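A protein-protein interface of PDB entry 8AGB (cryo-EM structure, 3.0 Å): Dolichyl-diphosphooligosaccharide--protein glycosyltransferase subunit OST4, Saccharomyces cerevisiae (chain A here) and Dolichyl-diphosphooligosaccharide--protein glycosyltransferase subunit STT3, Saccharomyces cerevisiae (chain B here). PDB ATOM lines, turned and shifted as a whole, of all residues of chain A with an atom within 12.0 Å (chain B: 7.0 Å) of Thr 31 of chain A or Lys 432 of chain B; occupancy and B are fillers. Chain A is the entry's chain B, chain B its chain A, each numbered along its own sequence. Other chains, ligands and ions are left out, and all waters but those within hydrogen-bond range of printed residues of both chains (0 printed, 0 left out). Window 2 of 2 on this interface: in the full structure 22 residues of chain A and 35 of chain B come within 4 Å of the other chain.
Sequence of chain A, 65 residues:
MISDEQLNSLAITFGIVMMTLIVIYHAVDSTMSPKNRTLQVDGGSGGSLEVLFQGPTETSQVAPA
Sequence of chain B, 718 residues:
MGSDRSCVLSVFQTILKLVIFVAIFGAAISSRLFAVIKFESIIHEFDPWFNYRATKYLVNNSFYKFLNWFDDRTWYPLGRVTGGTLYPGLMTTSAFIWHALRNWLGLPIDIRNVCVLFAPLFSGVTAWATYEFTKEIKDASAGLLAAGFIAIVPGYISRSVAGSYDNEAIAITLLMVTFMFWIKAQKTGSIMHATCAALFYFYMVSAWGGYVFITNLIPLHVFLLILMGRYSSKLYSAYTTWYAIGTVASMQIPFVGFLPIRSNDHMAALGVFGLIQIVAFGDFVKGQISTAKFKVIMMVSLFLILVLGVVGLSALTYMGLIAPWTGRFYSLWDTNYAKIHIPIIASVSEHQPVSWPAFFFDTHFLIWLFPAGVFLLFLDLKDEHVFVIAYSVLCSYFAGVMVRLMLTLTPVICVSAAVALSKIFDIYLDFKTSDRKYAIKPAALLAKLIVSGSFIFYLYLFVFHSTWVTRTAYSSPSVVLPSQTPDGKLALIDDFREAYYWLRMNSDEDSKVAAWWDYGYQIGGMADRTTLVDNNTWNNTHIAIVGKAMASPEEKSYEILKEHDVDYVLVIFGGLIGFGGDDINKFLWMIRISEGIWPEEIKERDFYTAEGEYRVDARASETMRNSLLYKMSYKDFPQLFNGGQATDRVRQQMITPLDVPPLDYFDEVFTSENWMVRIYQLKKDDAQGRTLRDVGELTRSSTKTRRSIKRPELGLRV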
ATOM      1  N   ILE A  22       3.832  14.698 -21.453  1.00  0.00           N
ATOM      2  CA  ILE A  22       3.853  15.154 -22.841  1.00  0.00           C
ATOM      3  C   ILE A  22       5.278  15.424 -23.305  1.00  0.00           C
ATOM      4  O   ILE A  22       5.662  15.048 -24.422  1.00  0.00           O
ATOM      5  CB  ILE A  22       2.953  16.391 -23.013  1.00  0.00           C
ATOM      6  CG1 ILE A  22       1.482  15.998 -22.882  1.00  0.00           C
ATOM      7  CG2 ILE A  22       3.201  17.047 -24.357  1.00  0.00           C
ATOM      8  CD1 ILE A  22       0.543  17.174 -22.835  1.00  0.00           C
ATOM      9  N   VAL A  23       6.098  16.058 -22.458  1.00  0.00           N
ATOM     10  CA  VAL A  23       7.471  16.339 -22.875  1.00  0.00           C
ATOM     11  C   VAL A  23       8.260  15.045 -23.048  1.00  0.00           C
ATOM     12  O   VAL A  23       9.041  14.900 -23.997  1.00  0.00           O
ATOM     13  CB  VAL A  23       8.163  17.292 -21.887  1.00  0.00           C
ATOM     14  CG1 VAL A  23       9.592  17.529 -22.315  1.00  0.00           C
ATOM     15  CG2 VAL A  23       7.436  18.614 -21.848  1.00  0.00           C
ATOM     16  N   ILE A  24       8.077  14.090 -22.133  1.00  0.00           N
ATOM     17  CA  ILE A  24       8.780  12.814 -22.246  1.00  0.00           C
ATOM     18  C   ILE A  24       8.370  12.087 -23.519  1.00  0.00           C
ATOM     19  O   ILE A  24       9.216  11.535 -24.236  1.00  0.00           O
ATOM     20  CB  ILE A  24       8.529  11.956 -20.994  1.00  0.00           C
ATOM     21  CG1 ILE A  24       9.218  12.576 -19.779  1.00  0.00           C
ATOM     22  CG2 ILE A  24       9.018  10.537 -21.214  1.00  0.00           C
ATOM     23  CD1 ILE A  24       9.083  11.758 -18.516  1.00  0.00           C
ATOM     24  N   TYR A  25       7.069  12.060 -23.811  1.00  0.00           N
ATOM     25  CA  TYR A  25       6.594  11.425 -25.036  1.00  0.00           C
ATOM     26  C   TYR A  25       7.202  12.077 -26.268  1.00  0.00           C
ATOM     27  O   TYR A  25       7.638  11.383 -27.193  1.00  0.00           O
ATOM     28  CB  TYR A  25       5.067  11.486 -25.096  1.00  0.00           C
ATOM     29  CG  TYR A  25       4.459  10.880 -26.341  1.00  0.00           C
ATOM     30  CD1 TYR A  25       4.300  11.626 -27.499  1.00  0.00           C
ATOM     31  CD2 TYR A  25       4.040   9.558 -26.354  1.00  0.00           C
ATOM     32  CE1 TYR A  25       3.745  11.072 -28.633  1.00  0.00           C
ATOM     33  CE2 TYR A  25       3.483   8.997 -27.483  1.00  0.00           C
ATOM     34  CZ  TYR A  25       3.339   9.760 -28.619  1.00  0.00           C
ATOM     35  OH  TYR A  25       2.784   9.205 -29.747  1.00  0.00           O
ATOM     36  N   HIS A  26       7.231  13.411 -26.302  1.00  0.00           N
ATOM     37  CA  HIS A  26       7.791  14.096 -27.461  1.00  0.00           C
ATOM     38  C   HIS A  26       9.272  13.789 -27.627  1.00  0.00           C
ATOM     39  O   HIS A  26       9.740  13.557 -28.746  1.00  0.00           O
ATOM     40  CB  HIS A  26       7.568  15.600 -27.347  1.00  0.00           C
ATOM     41  CG  HIS A  26       7.464  16.289 -28.669  1.00  0.00           C
ATOM     42  ND1 HIS A  26       6.345  16.990 -29.057  1.00  0.00           N
ATOM     43  CD2 HIS A  26       8.337  16.371 -29.701  1.00  0.00           C
ATOM     44  CE1 HIS A  26       6.534  17.480 -30.268  1.00  0.00           C
ATOM     45  NE2 HIS A  26       7.735  17.120 -30.681  1.00  0.00           N
ATOM     46  N   ALA A  27      10.027  13.784 -26.527  1.00  0.00           N
ATOM     47  CA  ALA A  27      11.448  13.454 -26.607  1.00  0.00           C
ATOM     48  C   ALA A  27      11.655  12.042 -27.139  1.00  0.00           C
ATOM     49  O   ALA A  27      12.467  11.820 -28.046  1.00  0.00           O
ATOM     50  CB  ALA A  27      12.101  13.612 -25.236  1.00  0.00           C
ATOM     51  N   VAL A  28      10.927  11.073 -26.580  1.00  0.00           N
ATOM     52  CA  VAL A  28      11.059   9.687 -27.025  1.00  0.00           C
ATOM     53  C   VAL A  28      10.729   9.563 -28.506  1.00  0.00           C
ATOM     54  O   VAL A  28      11.447   8.900 -29.264  1.00  0.00           O
ATOM     55  CB  VAL A  28      10.176   8.765 -26.164  1.00  0.00           C
ATOM     56  CG1 VAL A  28       9.730   7.552 -26.960  1.00  0.00           C
ATOM     57  CG2 VAL A  28      10.924   8.335 -24.918  1.00  0.00           C
ATOM     58  N   ASP A  29       9.644  10.203 -28.946  1.00  0.00           N
ATOM     59  CA  ASP A  29       9.212  10.048 -30.331  1.00  0.00           C
ATOM     60  C   ASP A  29      10.163  10.745 -31.296  1.00  0.00           C
ATOM     61  O   ASP A  29      10.387  10.261 -32.409  1.00  0.00           O
ATOM     62  CB  ASP A  29       7.793  10.584 -30.502  1.00  0.00           C
ATOM     63  CG  ASP A  29       7.303  10.484 -31.929  1.00  0.00           C
ATOM     64  OD1 ASP A  29       7.104   9.350 -32.412  1.00  0.00           O
ATOM     65  OD2 ASP A  29       7.118  11.538 -32.571  1.00  0.00           O
ATOM     66  N   SER A  30      10.728  11.883 -30.893  1.00  0.00           N
ATOM     67  CA  SER A  30      11.631  12.615 -31.771  1.00  0.00           C
ATOM     68  C   SER A  30      13.008  11.973 -31.849  1.00  0.00           C
ATOM     69  O   SER A  30      13.667  12.064 -32.890  1.00  0.00           O
ATOM     70  CB  SER A  30      11.759  14.063 -31.304  1.00  0.00           C
ATOM     71  OG  SER A  30      10.490  14.608 -31.002  1.00  0.00           O
ATOM     72  N   THR A  31      13.460  11.320 -30.778  1.00  0.00           N
ATOM     73  CA  THR A  31      14.789  10.720 -30.807  1.00  0.00           C
ATOM     74  C   THR A  31      14.799   9.335 -31.449  1.00  0.00           C
ATOM     75  O   THR A  31      15.821   8.938 -32.019  1.00  0.00           O
ATOM     76  CB  THR A  31      15.381  10.686 -29.393  1.00  0.00           C
ATOM     77  OG1 THR A  31      16.810  10.678 -29.472  1.00  0.00           O
ATOM     78  CG2 THR A  31      14.912   9.478 -28.618  1.00  0.00           C
ATOM     79  N   MET A  32      13.694   8.588 -31.387  1.00  0.00           N
ATOM     80  CA  MET A  32      13.661   7.213 -31.878  1.00  0.00           C
ATOM     81  C   MET A  32      12.849   7.061 -33.160  1.00  0.00           C
ATOM     82  O   MET A  32      12.431   5.949 -33.493  1.00  0.00           O
ATOM     83  CB  MET A  32      13.112   6.266 -30.808  1.00  0.00           C
ATOM     84  CG  MET A  32      13.853   6.296 -29.491  1.00  0.00           C
ATOM     85  SD  MET A  32      15.241   5.150 -29.454  1.00  0.00           S
ATOM     86  CE  MET A  32      15.589   5.100 -27.699  1.00  0.00           C
ATOM     87  N   SER A  33      12.618   8.147 -33.889  1.00  0.00           N
ATOM     88  CA  SER A  33      11.819   8.056 -35.106  1.00  0.00           C
ATOM     89  C   SER A  33      12.211   9.155 -36.085  1.00  0.00           C
ATOM     90  O   SER A  33      12.123  10.345 -35.754  1.00  0.00           O
ATOM     91  CB  SER A  33      10.327   8.138 -34.785  1.00  0.00           C
ATOM     92  OG  SER A  33       9.940   7.120 -33.877  1.00  0.00           O
ATOM     93  N   PRO A  34      12.648   8.797 -37.303  1.00  0.00           N
ATOM     94  CA  PRO A  34      13.087   9.752 -38.325  1.00  0.00           C
ATOM     95  C   PRO A  34      11.969  10.681 -38.786  1.00  0.00           C
ATOM     96  O   PRO A  34      12.255  11.818 -39.162  1.00  0.00           O
ATOM     97  CB  PRO A  34      13.550   8.848 -39.472  1.00  0.00           C
ATOM     98  CG  PRO A  34      12.798   7.580 -39.277  1.00  0.00           C
ATOM     99  CD  PRO A  34      12.680   7.409 -37.795  1.00  0.00           C
ATOM    100  N   ASP B 426      11.072  19.007 -32.372  1.00  0.00           N
ATOM    101  CA  ASP B 426      11.529  18.045 -33.368  1.00  0.00           C
ATOM    102  C   ASP B 426      13.003  18.223 -33.695  1.00  0.00           C
ATOM    103  O   ASP B 426      13.634  17.297 -34.216  1.00  0.00           O
ATOM    104  CB  ASP B 426      10.698  18.170 -34.645  1.00  0.00           C
ATOM    105  CG  ASP B 426       9.518  17.222 -34.668  1.00  0.00           C
ATOM    106  OD1 ASP B 426       9.593  16.162 -34.015  1.00  0.00           O
ATOM    107  OD2 ASP B 426       8.515  17.534 -35.341  1.00  0.00           O
ATOM    108  N   LEU B 429      14.875  18.325 -29.269  1.00  0.00           N
ATOM    109  CA  LEU B 429      14.759  17.151 -28.417  1.00  0.00           C
ATOM    110  C   LEU B 429      15.167  15.870 -29.128  1.00  0.00           C
ATOM    111  O   LEU B 429      15.160  14.804 -28.503  1.00  0.00           O
ATOM    112  CB  LEU B 429      13.332  16.992 -27.877  1.00  0.00           C
ATOM    113  CG  LEU B 429      12.871  17.935 -26.768  1.00  0.00           C
ATOM    114  CD1 LEU B 429      11.379  17.797 -26.575  1.00  0.00           C
ATOM    115  CD2 LEU B 429      13.604  17.643 -25.476  1.00  0.00           C
ATOM    116  N   ASP B 430      15.514  15.941 -30.410  1.00  0.00           N
ATOM    117  CA  ASP B 430      16.018  14.791 -31.157  1.00  0.00           C
ATOM    118  C   ASP B 430      17.516  14.698 -30.902  1.00  0.00           C
ATOM    119  O   ASP B 430      18.306  15.423 -31.509  1.00  0.00           O
ATOM    120  CB  ASP B 430      15.704  14.943 -32.640  1.00  0.00           C
ATOM    121  CG  ASP B 430      16.470  13.970 -33.499  1.00  0.00           C
ATOM    122  OD1 ASP B 430      16.370  12.756 -33.242  1.00  0.00           O
ATOM    123  OD2 ASP B 430      17.169  14.416 -34.432  1.00  0.00           O
ATOM    124  N   PHE B 431      17.914  13.783 -30.015  1.00  0.00           N
ATOM    125  CA  PHE B 431      19.305  13.722 -29.582  1.00  0.00           C
ATOM    126  C   PHE B 431      20.201  12.950 -30.543  1.00  0.00           C
ATOM    127  O   PHE B 431      21.394  13.254 -30.634  1.00  0.00           O
ATOM    128  CB  PHE B 431      19.385  13.101 -28.188  1.00  0.00           C
ATOM    129  CG  PHE B 431      18.874  13.998 -27.098  1.00  0.00           C
ATOM    130  CD1 PHE B 431      19.518  15.185 -26.801  1.00  0.00           C
ATOM    131  CD2 PHE B 431      17.749  13.654 -26.372  1.00  0.00           C
ATOM    132  CE1 PHE B 431      19.050  16.009 -25.800  1.00  0.00           C
ATOM    133  CE2 PHE B 431      17.276  14.476 -25.371  1.00  0.00           C
ATOM    134  CZ  PHE B 431      17.928  15.655 -25.085  1.00  0.00           C
ATOM    135  N   LYS B 432      19.668  11.956 -31.248  1.00  0.00           N
ATOM    136  CA  LYS B 432      20.476  11.154 -32.167  1.00  0.00           C
ATOM    137  C   LYS B 432      21.152  12.023 -33.224  1.00  0.00           C
ATOM    138  O   LYS B 432      22.378  12.123 -33.268  1.00  0.00           O
ATOM    139  CB  LYS B 432      19.629  10.079 -32.849  1.00  0.00           C
ATOM    140  CG  LYS B 432      18.529  10.626 -33.732  1.00  0.00           C
ATOM    141  CD  LYS B 432      18.297   9.749 -34.948  1.00  0.00           C
ATOM    142  CE  LYS B 432      17.010  10.133 -35.656  1.00  0.00           C
ATOM    143  NZ  LYS B 432      16.828  11.609 -35.708  1.00  0.00           N
ATOM    144  N   LYS B 448      21.071  22.035 -27.227  1.00  0.00           N
ATOM    145  CA  LYS B 448      19.754  21.415 -27.177  1.00  0.00           C
ATOM    146  C   LYS B 448      19.147  21.547 -25.789  1.00  0.00           C
ATOM    147  O   LYS B 448      17.955  21.860 -25.650  1.00  0.00           O
ATOM    148  CB  LYS B 448      19.866  19.946 -27.577  1.00  0.00           C
ATOM    149  CG  LYS B 448      20.090  19.731 -29.057  1.00  0.00           C
ATOM    150  CD  LYS B 448      20.633  18.343 -29.326  1.00  0.00           C
ATOM    151  CE  LYS B 448      20.043  17.757 -30.587  1.00  0.00           C
ATOM    152  NZ  LYS B 448      20.464  18.505 -31.798  1.00  0.00           N
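Printed residues of chain B within 4 Å of His 26 of chain A: Asp 426 (3.9 Å).
Of the printed residues of chain B, Ser 30 of chain A touches Asp 426 and Asp 430.
Thr 31 of chain A touches three residues of chain B.
Met 32 of chain A touches none of the printed residues of chain B.
Printed residues of chain A within 4 Å of Asp 426 of chain B: His 26 and Ser 30.
Phe 431 of chain B touches just one residue of chain A: Thr 31.
Lys 432 of chain B touches one residue of chain A.
The nearest residue of chain B that does not touch Thr 31 of chain A is Leu 429 of chain B (4.2 Å).
The nearest printed residue of chain A that does not touch Asp 426 of chain B is Asp 29 of chain A (5.4 Å).
The side-chain carboxylate (OD1) of Asp 430 of chain B is in salt-bridge range of the side-chain amino group (NZ) of Lys 432 of chain B.
The backbone carbonyl oxygen (O) of His 26 of chain A sits at hydrogen-bond distance from the side-chain hydroxyl (OG) of Ser 30 of chain A, at 2.6 Å.
Of the 13 printed residues of chain A, 3 touch a printed residue of chain B.
Of the 6 printed residues of chain B, 4 touch a printed residue of chain A.
Hydrophobic or aromatic side chains of chain B within 4 Å of the printed part of chain A: Phe 431.
Among the printed residues, no Asp or Glu carboxylate lies within 4 Å of a Lys or Arg side-chain nitrogen of the other chain.
Among the printed residues, pairs that only touch across the chains: His 26 of chain A with Asp 426 of chain B, Ser 30 of chain A with Asp 426 of chain B, Thr 31 of chain A with Asp 430 of chain B and Thr 31 of chain A with Lys 432 of chain B.
The backbone NH (N) of Phe 431 of chain B sits at hydrogen-bond distance from the side-chain hydroxyl (OG1) of Thr 31 of chain A (3.3 Å).
The side-chain carboxylate of Asp 430 of chain B sits close to the backbone carbonyl oxygen of Ser 30 of chain A, at 2.8 Å.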
